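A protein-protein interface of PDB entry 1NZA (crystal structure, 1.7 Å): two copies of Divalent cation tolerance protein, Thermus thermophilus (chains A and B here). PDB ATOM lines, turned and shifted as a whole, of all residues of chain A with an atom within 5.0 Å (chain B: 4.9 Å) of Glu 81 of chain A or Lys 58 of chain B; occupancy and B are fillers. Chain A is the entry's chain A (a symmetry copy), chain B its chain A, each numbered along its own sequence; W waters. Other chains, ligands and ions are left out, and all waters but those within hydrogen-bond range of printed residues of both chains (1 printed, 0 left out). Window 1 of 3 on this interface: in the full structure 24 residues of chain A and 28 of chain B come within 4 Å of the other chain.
Printed residues of chain B that touch a printed residue of chain A: Lys 58 and Tyr 94. Hydrophobic or aromatic side chains of chain B that line the printed part of chain A: Tyr 94. Of the 8 printed residues of chain A, 4 touch a printed residue of chain B. Hydrophobic or aromatic side chains of chain A within 4 Å of the printed part of chain B: Val 79 and Val 83. Among the printed residues, 5 pairs touch across the chains. Among the printed residues, Asp or Glu carboxylates within 4 Å of a Lys or Arg side-chain nitrogen of the other chain: Glu 81 of chain A with Lys 58 of chain B.
No position is printed for both chains.
Glu 81 of chain A touches two residues of chain B. Lys 58 of chain B touches just one residue of chain A: Glu 81. Of the printed residues of chain B, Val 83 of chain A touches Tyr 94 (3.7 Å). Of the printed residues of chain B, Pro 80 of chain A touches Tyr 94. Of the printed residues of chain B, Val 79 of chain A touches Tyr 94. Printed residues of chain A within 4 Å of Tyr 94 of chain B: Val 79 (3.6 Å), Pro 80 (3.7 Å), Glu 81 (3.4 Å) and Val 83 (3.7 Å). The nearest printed residue of chain B that does not touch Val 79 of chain A is Leu 98 of chain B (7.5 Å).
The backbone carbonyl oxygen (O) of Lys 58 of chain B is in hydrogen-bond range of the backbone NH (N) of Ala 29 of chain B, 3.1 Å away. N of Leu 6 of chain A is in hydrogen-bond range of O of Val 83 of chain A (2.8 Å). The side-chain hydroxyl (OG1) of Thr 8 of chain A sits at hydrogen-bond distance from the side-chain carboxylate (OE2) of Glu 81 of chain A, 2.8 Å away. The backbone NH of Lys 58 of chain B lies within hydrogen-bond range of the backbone carbonyl oxygen of Cys 30 of chain B. The side-chain amide oxygen (OD1) of Asn 32 of chain B sits at hydrogen-bond distance from the side-chain amino group (NZ) of Lys 58 of chain B, 2.7 Å away.
Water W1 lies within hydrogen-bond range of the side-chain carboxylate of Glu 81 of chain A (2.7 Å), the side-chain sulfur of Cys 30 of chain B (2.9 Å), the side-chain amide nitrogen of Asn 32 of chain B (3.2 Å) and the side-chain hydroxyl of Thr 8 of chain A (3.3 Å).
OE1 of Glu 81 of chain A lies within salt-bridge range of NZ of Lys 58 of chain B.
Tyr 94 of chain B touches Val 79 of chain A (CA to CG1, 3.6 Å). Tyr 94 of chain B touches Pro 80 of chain A (CB to O, 3.7 Å). CG of Glu 81 of chain A touches CZ of Tyr 94 of chain B (3.4 Å). Tyr 94 of chain B touches Val 83 of chain A.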
ATOM      1  N   LEU A   6      13.872   5.415  22.796  1.00  0.00           N
ATOM      2  CA  LEU A   6      14.006   3.970  22.953  1.00  0.00           C
ATOM      3  C   LEU A   6      14.396   3.360  21.614  1.00  0.00           C
ATOM      4  O   LEU A   6      13.841   3.720  20.573  1.00  0.00           O
ATOM      5  CB  LEU A   6      12.685   3.342  23.409  1.00  0.00           C
ATOM      6  CG  LEU A   6      12.000   3.907  24.657  1.00  0.00           C
ATOM      7  CD1 LEU A   6      10.826   3.012  25.046  1.00  0.00           C
ATOM      8  CD2 LEU A   6      12.983   3.995  25.785  1.00  0.00           C
ATOM      9  N   ILE A   7      15.343   2.429  21.649  1.00  0.00           N
ATOM     10  CA  ILE A   7      15.808   1.740  20.449  1.00  0.00           C
ATOM     11  C   ILE A   7      16.129   0.319  20.884  1.00  0.00           C
ATOM     12  O   ILE A   7      16.751   0.127  21.925  1.00  0.00           O
ATOM     13  CB  ILE A   7      17.125   2.347  19.901  1.00  0.00           C
ATOM     14  CG1 ILE A   7      16.943   3.833  19.581  1.00  0.00           C
ATOM     15  CG2 ILE A   7      17.557   1.601  18.632  1.00  0.00           C
ATOM     16  CD1 ILE A   7      18.244   4.546  19.287  1.00  0.00           C
ATOM     17  N   THR A   8      15.687  -0.677  20.130  1.00  0.00           N
ATOM     18  CA  THR A   8      16.048  -2.040  20.492  1.00  0.00           C
ATOM     19  C   THR A   8      17.004  -2.524  19.412  1.00  0.00           C
ATOM     20  O   THR A   8      16.909  -2.099  18.257  1.00  0.00           O
ATOM     21  CB  THR A   8      14.828  -2.963  20.598  1.00  0.00           C
ATOM     22  OG1 THR A   8      13.977  -2.766  19.467  1.00  0.00           O
ATOM     23  CG2 THR A   8      14.054  -2.668  21.880  1.00  0.00           C
ATOM     24  N   VAL A  79      13.872  -1.359   9.188  1.00  0.00           N
ATOM     25  CA  VAL A  79      12.965  -0.488   9.936  1.00  0.00           C
ATOM     26  C   VAL A  79      13.194  -0.642  11.436  1.00  0.00           C
ATOM     27  O   VAL A  79      12.408  -1.288  12.132  1.00  0.00           O
ATOM     28  CB  VAL A  79      11.489  -0.817   9.625  1.00  0.00           C
ATOM     29  CG1 VAL A  79      10.565   0.118  10.403  1.00  0.00           C
ATOM     30  CG2 VAL A  79      11.237  -0.685   8.130  1.00  0.00           C
ATOM     31  N   PRO A  80      14.275  -0.041  11.952  1.00  0.00           N
ATOM     32  CA  PRO A  80      14.583  -0.137  13.380  1.00  0.00           C
ATOM     33  C   PRO A  80      13.619   0.640  14.259  1.00  0.00           C
ATOM     34  O   PRO A  80      13.068   1.665  13.850  1.00  0.00           O
ATOM     35  CB  PRO A  80      15.998   0.420  13.458  1.00  0.00           C
ATOM     36  CG  PRO A  80      15.976   1.491  12.418  1.00  0.00           C
ATOM     37  CD  PRO A  80      15.264   0.807  11.263  1.00  0.00           C
ATOM     38  N   GLU A  81      13.411   0.144  15.471  1.00  0.00           N
ATOM     39  CA  GLU A  81      12.538   0.837  16.394  1.00  0.00           C
ATOM     40  C   GLU A  81      13.273   2.046  16.934  1.00  0.00           C
ATOM     41  O   GLU A  81      14.358   1.912  17.501  1.00  0.00           O
ATOM     42  CB  GLU A  81      12.158  -0.051  17.575  1.00  0.00           C
ATOM     43  CG  GLU A  81      11.443   0.729  18.675  1.00  0.00           C
ATOM     44  CD  GLU A  81      11.192  -0.089  19.918  1.00  0.00           C
ATOM     45  OE1 GLU A  81      10.373   0.352  20.749  1.00  0.00           O
ATOM     46  OE2 GLU A  81      11.813  -1.163  20.073  1.00  0.00           O
ATOM     47  N   ILE A  82      12.688   3.223  16.743  1.00  0.00           N
ATOM     48  CA  ILE A  82      13.249   4.467  17.257  1.00  0.00           C
ATOM     49  C   ILE A  82      12.054   5.310  17.679  1.00  0.00           C
ATOM     50  O   ILE A  82      11.398   5.923  16.835  1.00  0.00           O
ATOM     51  CB  ILE A  82      14.027   5.268  16.187  1.00  0.00           C
ATOM     52  CG1 ILE A  82      15.019   4.361  15.460  1.00  0.00           C
ATOM     53  CG2 ILE A  82      14.776   6.421  16.854  1.00  0.00           C
ATOM     54  CD1 ILE A  82      15.811   5.067  14.367  1.00  0.00           C
ATOM     55  N   VAL A  83      11.755   5.330  18.976  1.00  0.00           N
ATOM     56  CA  VAL A  83      10.624   6.108  19.468  1.00  0.00           C
ATOM     57  C   VAL A  83      11.071   7.057  20.569  1.00  0.00           C
ATOM     58  O   VAL A  83      11.802   6.666  21.477  1.00  0.00           O
ATOM     59  CB  VAL A  83       9.500   5.193  20.012  1.00  0.00           C
ATOM     60  CG1 VAL A  83       9.056   4.205  18.928  1.00  0.00           C
ATOM     61  CG2 VAL A  83       9.972   4.459  21.256  1.00  0.00           C
ATOM     62  N   GLU B   3       1.698   5.043  21.627  1.00  0.00           N
ATOM     63  CA  GLU B   3       2.107   5.033  23.027  1.00  0.00           C
ATOM     64  C   GLU B   3       2.974   3.841  23.379  1.00  0.00           C
ATOM     65  O   GLU B   3       2.939   2.816  22.700  1.00  0.00           O
ATOM     66  CB  GLU B   3       0.874   4.967  23.929  1.00  0.00           C
ATOM     67  CG  GLU B   3      -0.031   6.179  23.915  1.00  0.00           C
ATOM     68  CD  GLU B   3      -1.326   5.933  24.676  1.00  0.00           C
ATOM     69  OE1 GLU B   3      -1.826   6.878  25.320  1.00  0.00           O
ATOM     70  OE2 GLU B   3      -1.851   4.799  24.622  1.00  0.00           O
ATOM     71  N   VAL B   4       3.765   4.000  24.440  1.00  0.00           N
ATOM     72  CA  VAL B   4       4.581   2.909  24.966  1.00  0.00           C
ATOM     73  C   VAL B   4       3.929   2.651  26.322  1.00  0.00           C
ATOM     74  O   VAL B   4       3.973   3.503  27.217  1.00  0.00           O
ATOM     75  CB  VAL B   4       6.052   3.307  25.194  1.00  0.00           C
ATOM     76  CG1 VAL B   4       6.775   2.179  25.939  1.00  0.00           C
ATOM     77  CG2 VAL B   4       6.746   3.561  23.859  1.00  0.00           C
ATOM     78  N   ALA B  28      -1.449  -4.538  20.063  1.00  0.00           N
ATOM     79  CA  ALA B  28      -0.091  -4.023  20.163  1.00  0.00           C
ATOM     80  C   ALA B  28       0.678  -4.637  18.999  1.00  0.00           C
ATOM     81  O   ALA B  28       0.369  -5.751  18.570  1.00  0.00           O
ATOM     82  CB  ALA B  28       0.533  -4.428  21.492  1.00  0.00           C
ATOM     83  N   ALA B  29       1.661  -3.912  18.479  1.00  0.00           N
ATOM     84  CA  ALA B  29       2.449  -4.400  17.355  1.00  0.00           C
ATOM     85  C   ALA B  29       3.715  -5.072  17.856  1.00  0.00           C
ATOM     86  O   ALA B  29       4.261  -5.968  17.211  1.00  0.00           O
ATOM     87  CB  ALA B  29       2.819  -3.250  16.438  1.00  0.00           C
ATOM     88  N   CYS B  30       4.176  -4.629  19.018  1.00  0.00           N
ATOM     89  CA  CYS B  30       5.399  -5.168  19.598  1.00  0.00           C
ATOM     90  C   CYS B  30       5.350  -5.107  21.111  1.00  0.00           C
ATOM     91  O   CYS B  30       4.742  -4.202  21.685  1.00  0.00           O
ATOM     92  CB  CYS B  30       6.589  -4.355  19.095  1.00  0.00           C
ATOM     93  SG  CYS B  30       8.188  -4.826  19.793  1.00  0.00           S
ATOM     94  N   ASN B  32       8.092  -5.762  24.485  1.00  0.00           N
ATOM     95  CA  ASN B  32       9.425  -6.117  24.977  1.00  0.00           C
ATOM     96  C   ASN B  32       9.276  -6.572  26.421  1.00  0.00           C
ATOM     97  O   ASN B  32       8.596  -5.915  27.207  1.00  0.00           O
ATOM     98  CB  ASN B  32      10.371  -4.910  24.985  1.00  0.00           C
ATOM     99  CG  ASN B  32      10.514  -4.255  23.634  1.00  0.00           C
ATOM    100  OD1 ASN B  32      10.415  -3.033  23.523  1.00  0.00           O
ATOM    101  ND2 ASN B  32      10.767  -5.054  22.603  1.00  0.00           N
ATOM    102  N   LEU B  56       7.093  -3.656  27.900  1.00  0.00           N
ATOM    103  CA  LEU B  56       7.059  -2.353  27.219  1.00  0.00           C
ATOM    104  C   LEU B  56       6.221  -2.649  25.984  1.00  0.00           C
ATOM    105  O   LEU B  56       6.659  -3.369  25.087  1.00  0.00           O
ATOM    106  CB  LEU B  56       8.459  -1.894  26.803  1.00  0.00           C
ATOM    107  CG  LEU B  56       9.486  -1.638  27.908  1.00  0.00           C
ATOM    108  CD1 LEU B  56      10.766  -1.056  27.311  1.00  0.00           C
ATOM    109  CD2 LEU B  56       8.913  -0.680  28.906  1.00  0.00           C
ATOM    110  N   VAL B  57       5.013  -2.092  25.944  1.00  0.00           N
ATOM    111  CA  VAL B  57       4.076  -2.346  24.851  1.00  0.00           C
ATOM    112  C   VAL B  57       3.908  -1.187  23.873  1.00  0.00           C
ATOM    113  O   VAL B  57       3.545  -0.086  24.274  1.00  0.00           O
ATOM    114  CB  VAL B  57       2.683  -2.687  25.425  1.00  0.00           C
ATOM    115  CG1 VAL B  57       1.757  -3.160  24.309  1.00  0.00           C
ATOM    116  CG2 VAL B  57       2.817  -3.752  26.513  1.00  0.00           C
ATOM    117  N   LYS B  58       4.159  -1.446  22.590  1.00  0.00           N
ATOM    118  CA  LYS B  58       4.016  -0.420  21.552  1.00  0.00           C
ATOM    119  C   LYS B  58       2.591  -0.505  21.003  1.00  0.00           C
ATOM    120  O   LYS B  58       2.243  -1.457  20.305  1.00  0.00           O
ATOM    121  CB  LYS B  58       5.018  -0.672  20.428  1.00  0.00           C
ATOM    122  CG  LYS B  58       6.398  -1.089  20.915  1.00  0.00           C
ATOM    123  CD  LYS B  58       7.027  -0.055  21.830  1.00  0.00           C
ATOM    124  CE  LYS B  58       8.114  -0.697  22.672  1.00  0.00           C
ATOM    125  NZ  LYS B  58       9.022  -1.538  21.830  1.00  0.00           N
ATOM    126  N   THR B  59       1.773   0.499  21.301  1.00  0.00           N
ATOM    127  CA  THR B  59       0.381   0.477  20.862  1.00  0.00           C
ATOM    128  C   THR B  59      -0.144   1.880  20.536  1.00  0.00           C
ATOM    129  O   THR B  59       0.641   2.789  20.277  1.00  0.00           O
ATOM    130  CB  THR B  59      -0.483  -0.176  21.962  1.00  0.00           C
ATOM    131  OG1 THR B  59      -1.840  -0.303  21.519  1.00  0.00           O
ATOM    132  CG2 THR B  59      -0.425   0.653  23.230  1.00  0.00           C
ATOM    133  N   THR B  60      -1.467   2.043  20.531  1.00  0.00           N
ATOM    134  CA  THR B  60      -2.081   3.339  20.238  1.00  0.00           C
ATOM    135  C   THR B  60      -3.209   3.656  21.221  1.00  0.00           C
ATOM    136  O   THR B  60      -3.722   2.772  21.910  1.00  0.00           O
ATOM    137  CB  THR B  60      -2.676   3.376  18.816  1.00  0.00           C
ATOM    138  OG1 THR B  60      -3.825   2.524  18.760  1.00  0.00           O
ATOM    139  CG2 THR B  60      -1.661   2.900  17.800  1.00  0.00           C
ATOM    140  N   TYR B  94       8.647   3.121  11.247  1.00  0.00           N
ATOM    141  CA  TYR B  94       8.396   2.230  12.374  1.00  0.00           C
ATOM    142  C   TYR B  94       7.026   2.527  12.972  1.00  0.00           C
ATOM    143  O   TYR B  94       6.263   1.613  13.285  1.00  0.00           O
ATOM    144  CB  TYR B  94       9.464   2.397  13.461  1.00  0.00           C
ATOM    145  CG  TYR B  94       9.254   1.474  14.637  1.00  0.00           C
ATOM    146  CD1 TYR B  94       9.509   0.107  14.530  1.00  0.00           C
ATOM    147  CD2 TYR B  94       8.752   1.955  15.844  1.00  0.00           C
ATOM    148  CE1 TYR B  94       9.269  -0.761  15.597  1.00  0.00           C
ATOM    149  CE2 TYR B  94       8.507   1.097  16.915  1.00  0.00           C
ATOM    150  CZ  TYR B  94       8.769  -0.259  16.785  1.00  0.00           C
ATOM    151  OH  TYR B  94       8.542  -1.112  17.845  1.00  0.00           O
ATOM    152  N   LEU B  98       3.632   0.346  13.290  1.00  0.00           N
ATOM    153  CA  LEU B  98       2.989   0.239  14.591  1.00  0.00           C
ATOM    154  C   LEU B  98       1.478   0.434  14.467  1.00  0.00           C
ATOM    155  O   LEU B  98       0.700  -0.357  14.999  1.00  0.00           O
ATOM    156  CB  LEU B  98       3.593   1.274  15.550  1.00  0.00           C
ATOM    157  CG  LEU B  98       3.248   1.210  17.040  1.00  0.00           C
ATOM    158  CD1 LEU B  98       4.166   2.151  17.806  1.00  0.00           C
ATOM    159  CD2 LEU B  98       1.789   1.587  17.270  1.00  0.00           C
ATOM    160  N   THR B 102      -1.921  -2.410  14.586  1.00  0.00           N
ATOM    161  CA  THR B 102      -2.672  -2.253  15.823  1.00  0.00           C
ATOM    162  C   THR B 102      -4.121  -1.924  15.477  1.00  0.00           C
ATOM    163  O   THR B 102      -4.384  -1.156  14.554  1.00  0.00           O
ATOM    164  CB  THR B 102      -2.078  -1.120  16.699  1.00  0.00           C
ATOM    165  OG1 THR B 102      -0.727  -1.448  17.048  1.00  0.00           O
ATOM    166  CG2 THR B 102      -2.887  -0.947  17.973  1.00  0.00           C
HETATM  167  O   HOH W   1      10.854  -3.663  19.728  1.00  0.00           O
